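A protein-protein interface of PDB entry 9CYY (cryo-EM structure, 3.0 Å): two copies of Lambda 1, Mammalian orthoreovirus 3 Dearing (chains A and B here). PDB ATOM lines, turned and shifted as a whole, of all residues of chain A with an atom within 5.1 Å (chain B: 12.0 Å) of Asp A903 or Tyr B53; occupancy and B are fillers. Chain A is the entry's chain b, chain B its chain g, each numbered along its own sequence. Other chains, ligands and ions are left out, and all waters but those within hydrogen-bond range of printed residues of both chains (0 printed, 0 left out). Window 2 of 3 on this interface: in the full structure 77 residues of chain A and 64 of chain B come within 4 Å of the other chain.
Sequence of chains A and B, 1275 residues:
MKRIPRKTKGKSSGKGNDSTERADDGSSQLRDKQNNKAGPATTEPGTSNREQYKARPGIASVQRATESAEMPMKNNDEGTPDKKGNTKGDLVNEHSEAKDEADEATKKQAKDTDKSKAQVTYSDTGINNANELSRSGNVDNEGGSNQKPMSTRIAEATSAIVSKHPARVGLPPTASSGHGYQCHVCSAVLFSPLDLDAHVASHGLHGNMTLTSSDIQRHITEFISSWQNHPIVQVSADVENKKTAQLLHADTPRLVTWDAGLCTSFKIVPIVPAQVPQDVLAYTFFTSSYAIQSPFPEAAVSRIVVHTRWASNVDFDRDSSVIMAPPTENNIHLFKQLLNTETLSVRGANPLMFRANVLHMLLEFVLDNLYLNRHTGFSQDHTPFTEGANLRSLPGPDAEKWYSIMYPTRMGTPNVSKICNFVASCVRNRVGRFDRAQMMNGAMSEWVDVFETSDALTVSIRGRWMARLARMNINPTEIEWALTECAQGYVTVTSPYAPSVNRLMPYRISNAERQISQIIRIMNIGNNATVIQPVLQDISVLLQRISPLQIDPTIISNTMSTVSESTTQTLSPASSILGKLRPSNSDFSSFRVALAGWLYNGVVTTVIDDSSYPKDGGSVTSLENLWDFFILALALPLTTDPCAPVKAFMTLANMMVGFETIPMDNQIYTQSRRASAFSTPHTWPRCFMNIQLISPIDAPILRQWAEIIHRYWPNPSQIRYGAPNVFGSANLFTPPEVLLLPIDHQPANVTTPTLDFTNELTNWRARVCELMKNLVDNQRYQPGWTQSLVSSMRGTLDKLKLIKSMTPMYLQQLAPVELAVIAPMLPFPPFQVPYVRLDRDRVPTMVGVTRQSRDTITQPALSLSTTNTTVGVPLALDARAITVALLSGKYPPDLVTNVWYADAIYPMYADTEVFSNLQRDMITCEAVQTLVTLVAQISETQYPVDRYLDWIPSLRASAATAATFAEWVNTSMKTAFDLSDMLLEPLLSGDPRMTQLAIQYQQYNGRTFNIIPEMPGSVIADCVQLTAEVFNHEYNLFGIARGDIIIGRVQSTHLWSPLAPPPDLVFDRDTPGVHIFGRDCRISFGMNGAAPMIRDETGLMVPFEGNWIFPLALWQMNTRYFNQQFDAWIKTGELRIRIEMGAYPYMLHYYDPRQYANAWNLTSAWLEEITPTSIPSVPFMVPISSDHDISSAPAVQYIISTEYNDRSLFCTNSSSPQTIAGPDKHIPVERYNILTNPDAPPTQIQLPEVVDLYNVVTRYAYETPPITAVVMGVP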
ATOM      1  N   TRP A 227     -21.136  -1.699 -10.780  1.00  0.00           N
ATOM      2  CA  TRP A 227     -20.788  -0.884  -9.626  1.00  0.00           C
ATOM      3  C   TRP A 227     -19.399  -0.273  -9.720  1.00  0.00           C
ATOM      4  O   TRP A 227     -18.951   0.356  -8.756  1.00  0.00           O
ATOM      5  CB  TRP A 227     -20.905  -1.705  -8.339  1.00  0.00           C
ATOM      6  CG  TRP A 227     -19.900  -2.801  -8.217  1.00  0.00           C
ATOM      7  CD1 TRP A 227     -18.655  -2.713  -7.674  1.00  0.00           C
ATOM      8  CD2 TRP A 227     -20.062  -4.160  -8.633  1.00  0.00           C
ATOM      9  NE1 TRP A 227     -18.025  -3.930  -7.732  1.00  0.00           N
ATOM     10  CE2 TRP A 227     -18.869  -4.836  -8.318  1.00  0.00           C
ATOM     11  CE3 TRP A 227     -21.096  -4.869  -9.247  1.00  0.00           C
ATOM     12  CZ2 TRP A 227     -18.684  -6.186  -8.593  1.00  0.00           C
ATOM     13  CZ3 TRP A 227     -20.910  -6.209  -9.518  1.00  0.00           C
ATOM     14  CH2 TRP A 227     -19.713  -6.854  -9.193  1.00  0.00           C
ATOM     15  N   GLN A 228     -18.706  -0.438 -10.842  1.00  0.00           N
ATOM     16  CA  GLN A 228     -17.381   0.140 -11.015  1.00  0.00           C
ATOM     17  C   GLN A 228     -17.086   0.229 -12.503  1.00  0.00           C
ATOM     18  O   GLN A 228     -17.822  -0.302 -13.336  1.00  0.00           O
ATOM     19  CB  GLN A 228     -16.310  -0.682 -10.294  1.00  0.00           C
ATOM     20  CG  GLN A 228     -16.236  -2.125 -10.741  1.00  0.00           C
ATOM     21  CD  GLN A 228     -15.377  -2.969  -9.827  1.00  0.00           C
ATOM     22  OE1 GLN A 228     -14.620  -2.445  -9.013  1.00  0.00           O
ATOM     23  NE2 GLN A 228     -15.492  -4.284  -9.954  1.00  0.00           N
ATOM     24  N   VAL A 899     -21.330  -7.681  -0.300  1.00  0.00           N
ATOM     25  CA  VAL A 899     -20.268  -6.871  -0.890  1.00  0.00           C
ATOM     26  C   VAL A 899     -19.054  -7.734  -1.209  1.00  0.00           C
ATOM     27  O   VAL A 899     -18.462  -7.630  -2.290  1.00  0.00           O
ATOM     28  CB  VAL A 899     -19.897  -5.708   0.045  1.00  0.00           C
ATOM     29  CG1 VAL A 899     -18.835  -4.836  -0.594  1.00  0.00           C
ATOM     30  CG2 VAL A 899     -21.123  -4.889   0.378  1.00  0.00           C
ATOM     31  N   TRP A 900     -18.665  -8.598  -0.270  1.00  0.00           N
ATOM     32  CA  TRP A 900     -17.429  -9.358  -0.427  1.00  0.00           C
ATOM     33  C   TRP A 900     -17.513 -10.319  -1.606  1.00  0.00           C
ATOM     34  O   TRP A 900     -16.599 -10.383  -2.435  1.00  0.00           O
ATOM     35  CB  TRP A 900     -17.115 -10.115   0.863  1.00  0.00           C
ATOM     36  CG  TRP A 900     -15.892 -10.977   0.781  1.00  0.00           C
ATOM     37  CD1 TRP A 900     -15.783 -12.200   0.187  1.00  0.00           C
ATOM     38  CD2 TRP A 900     -14.601 -10.678   1.317  1.00  0.00           C
ATOM     39  NE1 TRP A 900     -14.503 -12.678   0.318  1.00  0.00           N
ATOM     40  CE2 TRP A 900     -13.758 -11.761   1.009  1.00  0.00           C
ATOM     41  CE3 TRP A 900     -14.075  -9.596   2.029  1.00  0.00           C
ATOM     42  CZ2 TRP A 900     -12.421 -11.794   1.386  1.00  0.00           C
ATOM     43  CZ3 TRP A 900     -12.750  -9.632   2.402  1.00  0.00           C
ATOM     44  CH2 TRP A 900     -11.936 -10.723   2.080  1.00  0.00           C
ATOM     45  N   TYR A 901     -18.602 -11.081  -1.695  1.00  0.00           N
ATOM     46  CA  TYR A 901     -18.676 -12.126  -2.708  1.00  0.00           C
ATOM     47  C   TYR A 901     -18.967 -11.561  -4.090  1.00  0.00           C
ATOM     48  O   TYR A 901     -18.657 -12.207  -5.097  1.00  0.00           O
ATOM     49  CB  TYR A 901     -19.720 -13.165  -2.310  1.00  0.00           C
ATOM     50  CG  TYR A 901     -19.175 -14.177  -1.333  1.00  0.00           C
ATOM     51  CD1 TYR A 901     -17.986 -14.840  -1.592  1.00  0.00           C
ATOM     52  CD2 TYR A 901     -19.836 -14.456  -0.148  1.00  0.00           C
ATOM     53  CE1 TYR A 901     -17.475 -15.761  -0.705  1.00  0.00           C
ATOM     54  CE2 TYR A 901     -19.332 -15.377   0.747  1.00  0.00           C
ATOM     55  CZ  TYR A 901     -18.150 -16.026   0.463  1.00  0.00           C
ATOM     56  OH  TYR A 901     -17.640 -16.945   1.349  1.00  0.00           O
ATOM     57  N   ALA A 902     -19.563 -10.371  -4.166  1.00  0.00           N
ATOM     58  CA  ALA A 902     -19.699  -9.709  -5.458  1.00  0.00           C
ATOM     59  C   ALA A 902     -18.337  -9.329  -6.022  1.00  0.00           C
ATOM     60  O   ALA A 902     -18.093  -9.470  -7.225  1.00  0.00           O
ATOM     61  CB  ALA A 902     -20.591  -8.476  -5.328  1.00  0.00           C
ATOM     62  N   ASP A 903     -17.436  -8.848  -5.164  1.00  0.00           N
ATOM     63  CA  ASP A 903     -16.098  -8.461  -5.590  1.00  0.00           C
ATOM     64  C   ASP A 903     -15.215  -9.653  -5.930  1.00  0.00           C
ATOM     65  O   ASP A 903     -14.175  -9.465  -6.568  1.00  0.00           O
ATOM     66  CB  ASP A 903     -15.425  -7.627  -4.501  1.00  0.00           C
ATOM     67  CG  ASP A 903     -15.702  -6.147  -4.651  1.00  0.00           C
ATOM     68  OD1 ASP A 903     -16.355  -5.761  -5.641  1.00  0.00           O
ATOM     69  OD2 ASP A 903     -15.267  -5.370  -3.776  1.00  0.00           O
ATOM     70  N   ALA A 904     -15.588 -10.860  -5.513  1.00  0.00           N
ATOM     71  CA  ALA A 904     -14.795 -12.054  -5.777  1.00  0.00           C
ATOM     72  C   ALA A 904     -15.263 -12.822  -7.003  1.00  0.00           C
ATOM     73  O   ALA A 904     -14.433 -13.343  -7.754  1.00  0.00           O
ATOM     74  CB  ALA A 904     -14.817 -12.981  -4.560  1.00  0.00           C
ATOM     75  N   ILE A 905     -16.574 -12.910  -7.219  1.00  0.00           N
ATOM     76  CA  ILE A 905     -17.093 -13.688  -8.340  1.00  0.00           C
ATOM     77  C   ILE A 905     -16.792 -13.002  -9.666  1.00  0.00           C
ATOM     78  O   ILE A 905     -16.419 -13.656 -10.646  1.00  0.00           O
ATOM     79  CB  ILE A 905     -18.599 -13.940  -8.156  1.00  0.00           C
ATOM     80  CG1 ILE A 905     -18.831 -14.984  -7.064  1.00  0.00           C
ATOM     81  CG2 ILE A 905     -19.237 -14.384  -9.457  1.00  0.00           C
ATOM     82  CD1 ILE A 905     -20.210 -14.933  -6.460  1.00  0.00           C
ATOM     83  N   TYR A 906     -16.938 -11.677  -9.719  1.00  0.00           N
ATOM     84  CA  TYR A 906     -16.836 -10.942 -10.977  1.00  0.00           C
ATOM     85  C   TYR A 906     -15.485 -11.125 -11.668  1.00  0.00           C
ATOM     86  O   TYR A 906     -15.462 -11.467 -12.857  1.00  0.00           O
ATOM     87  CB  TYR A 906     -17.117  -9.455 -10.752  1.00  0.00           C
ATOM     88  CG  TYR A 906     -16.807  -8.595 -11.953  1.00  0.00           C
ATOM     89  CD1 TYR A 906     -17.387  -8.854 -13.186  1.00  0.00           C
ATOM     90  CD2 TYR A 906     -15.925  -7.530 -11.856  1.00  0.00           C
ATOM     91  CE1 TYR A 906     -17.103  -8.073 -14.285  1.00  0.00           C
ATOM     92  CE2 TYR A 906     -15.635  -6.744 -12.950  1.00  0.00           C
ATOM     93  CZ  TYR A 906     -16.226  -7.020 -14.161  1.00  0.00           C
ATOM     94  OH  TYR A 906     -15.940  -6.238 -15.253  1.00  0.00           O
ATOM     95  N   PRO A 907     -14.345 -10.905 -11.000  1.00  0.00           N
ATOM     96  CA  PRO A 907     -13.070 -11.171 -11.686  1.00  0.00           C
ATOM     97  C   PRO A 907     -12.885 -12.632 -12.044  1.00  0.00           C
ATOM     98  O   PRO A 907     -12.249 -12.946 -13.058  1.00  0.00           O
ATOM     99  CB  PRO A 907     -12.020 -10.694 -10.673  1.00  0.00           C
ATOM    100  CG  PRO A 907     -12.695 -10.773  -9.368  1.00  0.00           C
ATOM    101  CD  PRO A 907     -14.119 -10.410  -9.629  1.00  0.00           C
ATOM    102  N   SER B  48     -19.790  10.859 -16.137  1.00  0.00           N
ATOM    103  CA  SER B  48     -18.483  11.251 -15.637  1.00  0.00           C
ATOM    104  C   SER B  48     -17.840  10.100 -14.867  1.00  0.00           C
ATOM    105  O   SER B  48     -18.442   9.043 -14.653  1.00  0.00           O
ATOM    106  CB  SER B  48     -18.601  12.499 -14.766  1.00  0.00           C
ATOM    107  OG  SER B  48     -17.340  12.861 -14.232  1.00  0.00           O
ATOM    108  N   ASN B  49     -16.594  10.307 -14.438  1.00  0.00           N
ATOM    109  CA  ASN B  49     -15.842   9.319 -13.667  1.00  0.00           C
ATOM    110  C   ASN B  49     -15.344   9.986 -12.385  1.00  0.00           C
ATOM    111  O   ASN B  49     -14.232  10.512 -12.323  1.00  0.00           O
ATOM    112  CB  ASN B  49     -14.687   8.739 -14.483  1.00  0.00           C
ATOM    113  CG  ASN B  49     -15.108   8.325 -15.876  1.00  0.00           C
ATOM    114  OD1 ASN B  49     -16.162   7.717 -16.064  1.00  0.00           O
ATOM    115  ND2 ASN B  49     -14.284   8.651 -16.865  1.00  0.00           N
ATOM    116  N   ARG B  50     -16.184   9.958 -11.351  1.00  0.00           N
ATOM    117  CA  ARG B  50     -15.842  10.544 -10.064  1.00  0.00           C
ATOM    118  C   ARG B  50     -15.820   9.529  -8.931  1.00  0.00           C
ATOM    119  O   ARG B  50     -15.299   9.838  -7.854  1.00  0.00           O
ATOM    120  CB  ARG B  50     -16.828  11.664  -9.714  1.00  0.00           C
ATOM    121  CG  ARG B  50     -16.782  12.850 -10.662  1.00  0.00           C
ATOM    122  CD  ARG B  50     -17.899  13.837 -10.365  1.00  0.00           C
ATOM    123  NE  ARG B  50     -17.779  14.409  -9.030  1.00  0.00           N
ATOM    124  CZ  ARG B  50     -17.047  15.475  -8.734  1.00  0.00           C
ATOM    125  NH1 ARG B  50     -16.357  16.118  -9.662  1.00  0.00           N
ATOM    126  NH2 ARG B  50     -17.006  15.904  -7.477  1.00  0.00           N
ATOM    127  N   GLU B  51     -16.372   8.339  -9.146  1.00  0.00           N
ATOM    128  CA  GLU B  51     -16.392   7.323  -8.104  1.00  0.00           C
ATOM    129  C   GLU B  51     -14.983   6.817  -7.824  1.00  0.00           C
ATOM    130  O   GLU B  51     -14.201   6.560  -8.743  1.00  0.00           O
ATOM    131  CB  GLU B  51     -17.300   6.165  -8.520  1.00  0.00           C
ATOM    132  CG  GLU B  51     -17.192   4.936  -7.639  1.00  0.00           C
ATOM    133  CD  GLU B  51     -17.952   3.752  -8.200  1.00  0.00           C
ATOM    134  OE1 GLU B  51     -18.294   3.781  -9.400  1.00  0.00           O
ATOM    135  OE2 GLU B  51     -18.205   2.794  -7.441  1.00  0.00           O
ATOM    136  N   GLN B  52     -14.661   6.673  -6.539  1.00  0.00           N
ATOM    137  CA  GLN B  52     -13.362   6.171  -6.092  1.00  0.00           C
ATOM    138  C   GLN B  52     -13.622   4.955  -5.210  1.00  0.00           C
ATOM    139  O   GLN B  52     -13.731   5.075  -3.988  1.00  0.00           O
ATOM    140  CB  GLN B  52     -12.580   7.251  -5.354  1.00  0.00           C
ATOM    141  CG  GLN B  52     -12.190   8.429  -6.226  1.00  0.00           C
ATOM    142  CD  GLN B  52     -11.268   8.030  -7.360  1.00  0.00           C
ATOM    143  OE1 GLN B  52     -11.664   8.024  -8.526  1.00  0.00           O
ATOM    144  NE2 GLN B  52     -10.028   7.693  -7.023  1.00  0.00           N
ATOM    145  N   TYR B  53     -13.720   3.783  -5.832  1.00  0.00           N
ATOM    146  CA  TYR B  53     -14.011   2.539  -5.131  1.00  0.00           C
ATOM    147  C   TYR B  53     -12.798   1.627  -5.210  1.00  0.00           C
ATOM    148  O   TYR B  53     -12.276   1.376  -6.302  1.00  0.00           O
ATOM    149  CB  TYR B  53     -15.235   1.845  -5.727  1.00  0.00           C
ATOM    150  CG  TYR B  53     -15.550   0.520  -5.075  1.00  0.00           C
ATOM    151  CD1 TYR B  53     -15.665   0.416  -3.698  1.00  0.00           C
ATOM    152  CD2 TYR B  53     -15.736  -0.624  -5.836  1.00  0.00           C
ATOM    153  CE1 TYR B  53     -15.952  -0.790  -3.096  1.00  0.00           C
ATOM    154  CE2 TYR B  53     -16.022  -1.834  -5.243  1.00  0.00           C
ATOM    155  CZ  TYR B  53     -16.129  -1.910  -3.874  1.00  0.00           C
ATOM    156  OH  TYR B  53     -16.416  -3.116  -3.278  1.00  0.00           O
ATOM    157  N   LYS B  54     -12.355   1.133  -4.059  1.00  0.00           N
ATOM    158  CA  LYS B  54     -11.273   0.162  -3.982  1.00  0.00           C
ATOM    159  C   LYS B  54     -11.869  -1.178  -3.570  1.00  0.00           C
ATOM    160  O   LYS B  54     -12.319  -1.337  -2.430  1.00  0.00           O
ATOM    161  CB  LYS B  54     -10.199   0.626  -2.997  1.00  0.00           C
ATOM    162  CG  LYS B  54      -9.000  -0.305  -2.848  1.00  0.00           C
ATOM    163  CD  LYS B  54      -9.172  -1.281  -1.695  1.00  0.00           C
ATOM    164  CE  LYS B  54      -9.080  -0.569  -0.356  1.00  0.00           C
ATOM    165  NZ  LYS B  54      -9.234  -1.516   0.782  1.00  0.00           N
ATOM    166  N   ALA B  55     -11.872  -2.133  -4.495  1.00  0.00           N
ATOM    167  CA  ALA B  55     -12.544  -3.408  -4.292  1.00  0.00           C
ATOM    168  C   ALA B  55     -11.704  -4.323  -3.411  1.00  0.00           C
ATOM    169  O   ALA B  55     -10.482  -4.399  -3.570  1.00  0.00           O
ATOM    170  CB  ALA B  55     -12.825  -4.084  -5.634  1.00  0.00           C
ATOM    171  N   ARG B  56     -12.364  -5.013  -2.484  1.00  0.00           N
ATOM    172  CA  ARG B  56     -11.723  -6.012  -1.638  1.00  0.00           C
ATOM    173  C   ARG B  56     -12.554  -7.285  -1.720  1.00  0.00           C
ATOM    174  O   ARG B  56     -13.754  -7.258  -1.379  1.00  0.00           O
ATOM    175  CB  ARG B  56     -11.597  -5.524  -0.194  1.00  0.00           C
ATOM    176  CG  ARG B  56     -11.459  -6.637   0.827  1.00  0.00           C
ATOM    177  CD  ARG B  56     -11.363  -6.084   2.236  1.00  0.00           C
ATOM    178  NE  ARG B  56     -12.663  -6.024   2.892  1.00  0.00           N
ATOM    179  CZ  ARG B  56     -12.852  -5.640   4.147  1.00  0.00           C
ATOM    180  NH1 ARG B  56     -11.841  -5.274   4.916  1.00  0.00           N
ATOM    181  NH2 ARG B  56     -14.086  -5.622   4.640  1.00  0.00           N
ATOM    182  N   PRO B  57     -11.984  -8.418  -2.161  1.00  0.00           N
ATOM    183  CA  PRO B  57     -10.592  -8.630  -2.578  1.00  0.00           C
ATOM    184  C   PRO B  57     -10.216  -7.891  -3.859  1.00  0.00           C
ATOM    185  O   PRO B  57     -11.084  -7.596  -4.676  1.00  0.00           O
ATOM    186  CB  PRO B  57     -10.524 -10.144  -2.804  1.00  0.00           C
ATOM    187  CG  PRO B  57     -11.657 -10.700  -2.021  1.00  0.00           C
ATOM    188  CD  PRO B  57     -12.737  -9.682  -2.150  1.00  0.00           C
ATOM    189  N   GLY B  58      -8.927  -7.599  -4.019  1.00  0.00           N
ATOM    190  CA  GLY B  58      -8.479  -6.851  -5.176  1.00  0.00           C
ATOM    191  C   GLY B  58      -8.628  -7.633  -6.467  1.00  0.00           C
ATOM    192  O   GLY B  58      -8.531  -8.857  -6.500  1.00  0.00           O
ATOM    193  N   ILE B  59      -8.873  -6.895  -7.551  1.00  0.00           N
ATOM    194  CA  ILE B  59      -9.051  -7.524  -8.857  1.00  0.00           C
ATOM    195  C   ILE B  59      -7.759  -8.198  -9.304  1.00  0.00           C
ATOM    196  O   ILE B  59      -7.771  -9.315  -9.832  1.00  0.00           O
ATOM    197  CB  ILE B  59      -9.535  -6.490  -9.888  1.00  0.00           C
ATOM    198  CG1 ILE B  59     -10.906  -5.945  -9.489  1.00  0.00           C
ATOM    199  CG2 ILE B  59      -9.602  -7.105 -11.271  1.00  0.00           C
ATOM    200  CD1 ILE B  59     -11.339  -4.748 -10.297  1.00  0.00           C
ATOM    201  N   ALA B  60      -6.626  -7.525  -9.102  1.00  0.00           N
ATOM    202  CA  ALA B  60      -5.349  -8.067  -9.555  1.00  0.00           C
ATOM    203  C   ALA B  60      -5.015  -9.371  -8.843  1.00  0.00           C
ATOM    204  O   ALA B  60      -4.577 -10.341  -9.473  1.00  0.00           O
ATOM    205  CB  ALA B  60      -4.239  -7.039  -9.344  1.00  0.00           C
ATOM    206  N   SER B  61      -5.214  -9.415  -7.525  1.00  0.00           N
ATOM    207  CA  SER B  61      -4.862 -10.608  -6.762  1.00  0.00           C
ATOM    208  C   SER B  61      -5.714 -11.800  -7.178  1.00  0.00           C
ATOM    209  O   SER B  61      -5.209 -12.920  -7.318  1.00  0.00           O
ATOM    210  CB  SER B  61      -5.007 -10.336  -5.265  1.00  0.00           C
ATOM    211  OG  SER B  61      -6.363 -10.126  -4.919  1.00  0.00           O
ATOM    212  N   VAL B  62      -7.015 -11.580  -7.373  1.00  0.00           N
ATOM    213  CA  VAL B  62      -7.896 -12.670  -7.778  1.00  0.00           C
ATOM    214  C   VAL B  62      -7.551 -13.146  -9.183  1.00  0.00           C
ATOM    215  O   VAL B  62      -7.548 -14.350  -9.460  1.00  0.00           O
ATOM    216  CB  VAL B  62      -9.368 -12.238  -7.670  1.00  0.00           C
ATOM    217  CG1 VAL B  62     -10.282 -13.369  -8.096  1.00  0.00           C
ATOM    218  CG2 VAL B  62      -9.687 -11.817  -6.251  1.00  0.00           C
ATOM    219  N   GLN B  63      -7.252 -12.213 -10.089  1.00  0.00           N
ATOM    220  CA  GLN B  63      -6.962 -12.592 -11.469  1.00  0.00           C
ATOM    221  C   GLN B  63      -5.721 -13.469 -11.560  1.00  0.00           C
ATOM    222  O   GLN B  63      -5.680 -14.414 -12.354  1.00  0.00           O
ATOM    223  CB  GLN B  63      -6.796 -11.344 -12.335  1.00  0.00           C
ATOM    224  CG  GLN B  63      -8.050 -10.946 -13.084  1.00  0.00           C
ATOM    225  CD  GLN B  63      -7.945  -9.567 -13.694  1.00  0.00           C
ATOM    226  OE1 GLN B  63      -7.380  -8.653 -13.098  1.00  0.00           O
ATOM    227  NE2 GLN B  63      -8.489  -9.409 -14.895  1.00  0.00           N
ATOM    228  N   ARG B  64      -4.696 -13.167 -10.760  1.00  0.00           N
ATOM    229  CA  ARG B  64      -3.470 -13.957 -10.804  1.00  0.00           C
ATOM    230  C   ARG B  64      -3.731 -15.399 -10.389  1.00  0.00           C
ATOM    231  O   ARG B  64      -3.197 -16.338 -10.991  1.00  0.00           O
ATOM    232  CB  ARG B  64      -2.406 -13.326  -9.908  1.00  0.00           C
ATOM    233  CG  ARG B  64      -1.908 -11.981 -10.393  1.00  0.00           C
ATOM    234  CD  ARG B  64      -0.833 -11.431  -9.474  1.00  0.00           C
ATOM    235  NE  ARG B  64      -0.407 -10.097  -9.876  1.00  0.00           N
ATOM    236  CZ  ARG B  64       0.566  -9.848 -10.740  1.00  0.00           C
ATOM    237  NH1 ARG B  64       1.244 -10.828 -11.318  1.00  0.00           N
ATOM    238  NH2 ARG B  64       0.868  -8.587 -11.034  1.00  0.00           N
ATOM    239  N   ALA B  65      -4.551 -15.594  -9.355  1.00  0.00           N
ATOM    240  CA  ALA B  65      -4.820 -16.942  -8.870  1.00  0.00           C
ATOM    241  C   ALA B  65      -5.608 -17.758  -9.888  1.00  0.00           C
ATOM    242  O   ALA B  65      -5.351 -18.954 -10.063  1.00  0.00           O
ATOM    243  CB  ALA B  65      -5.567 -16.880  -7.539  1.00  0.00           C
ATOM    244  N   THR B  66      -6.573 -17.133 -10.567  1.00  0.00           N
ATOM    245  CA  THR B  66      -7.407 -17.876 -11.507  1.00  0.00           C
ATOM    246  C   THR B  66      -6.614 -18.316 -12.730  1.00  0.00           C
ATOM    247  O   THR B  66      -6.949 -19.323 -13.365  1.00  0.00           O
ATOM    248  CB  THR B  66      -8.610 -17.036 -11.930  1.00  0.00           C
ATOM    249  OG1 THR B  66      -8.161 -15.871 -12.630  1.00  0.00           O
ATOM    250  CG2 THR B  66      -9.420 -16.618 -10.719  1.00  0.00           C
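The side-chain carboxylate (OD2) of Asp A903 sits at hydrogen-bond distance from the side-chain hydroxyl (OH) of Tyr B53 (2.6 Å). The side-chain carboxylate (OD2) of Asp A903 is in hydrogen-bond range of the backbone NH (N) of Arg B56, 3.2 Å away. The side-chain carboxylate of Glu B51 lies close to the backbone carbonyl oxygen of Trp A227 (2.9 Å).
The indole nitrogen (NE1) of Trp A227 lies close to the side-chain amide nitrogen (NE2) of Gln A228. The side-chain carboxylate (OD1) of Asp A903 is in hydrogen-bond range of the indole nitrogen (NE1) of Trp A227, 3.2 Å away.
Among the printed residues, pairs that only touch across the chains: Trp A227 with Tyr B53 (3.7 Å), Gln A228 with Tyr B53 (3.8 Å), Trp A900 with Arg B56 (3.6 Å), Trp A900 with Pro B57 (3.7 Å), Asp A903 with Ala B55 (3.3 Å) and Pro A907 with Val B62 (3.8 Å).
Trp A227 touches two residues of chain B. Printed residues of chain B within 4 Å of Trp A900: Arg B56 and Pro B57. Of the printed residues of chain B, Asp A903 touches Tyr B53 (2.6 Å), Ala B55 (3.3 Å) and Arg B56 (3.2 Å). Printed residues of chain B within 4 Å of Pro A907: Val B62 (3.8 Å). Asn B49 touches none of the printed residues of chain A. Gln B52 touches none of the printed residues of chain A. Printed residues of chain A within 4 Å of Tyr B53: Trp A227, Gln A228 and Asp A903. Of the printed residues of chain A, Ala B55 touches Asp A903 (3.3 Å). Of the printed residues of chain A, Arg B56 touches Trp A900 (3.6 Å) and Asp A903 (3.2 Å). Of the printed residues of chain A, Pro B57 touches Trp A900. Of the printed residues of chain A, Val B62 touches Pro A907. The nearest residue of chain B that does not touch Asp A903 is Pro B57 (4.1 Å).
Hydrophobic or aromatic side chains of chain B within 4 Å of the printed part of chain A: Tyr B53, Ala B55, Pro B57 and Val B62. Among the printed residues, no Asp or Glu carboxylate lies within 4 Å of a Lys or Arg side-chain nitrogen of the other chain.
No position is printed for both chains. Of the 9 pairs that touch across the chains among the printed residues, none has its exchanged pair printed and touching as well.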
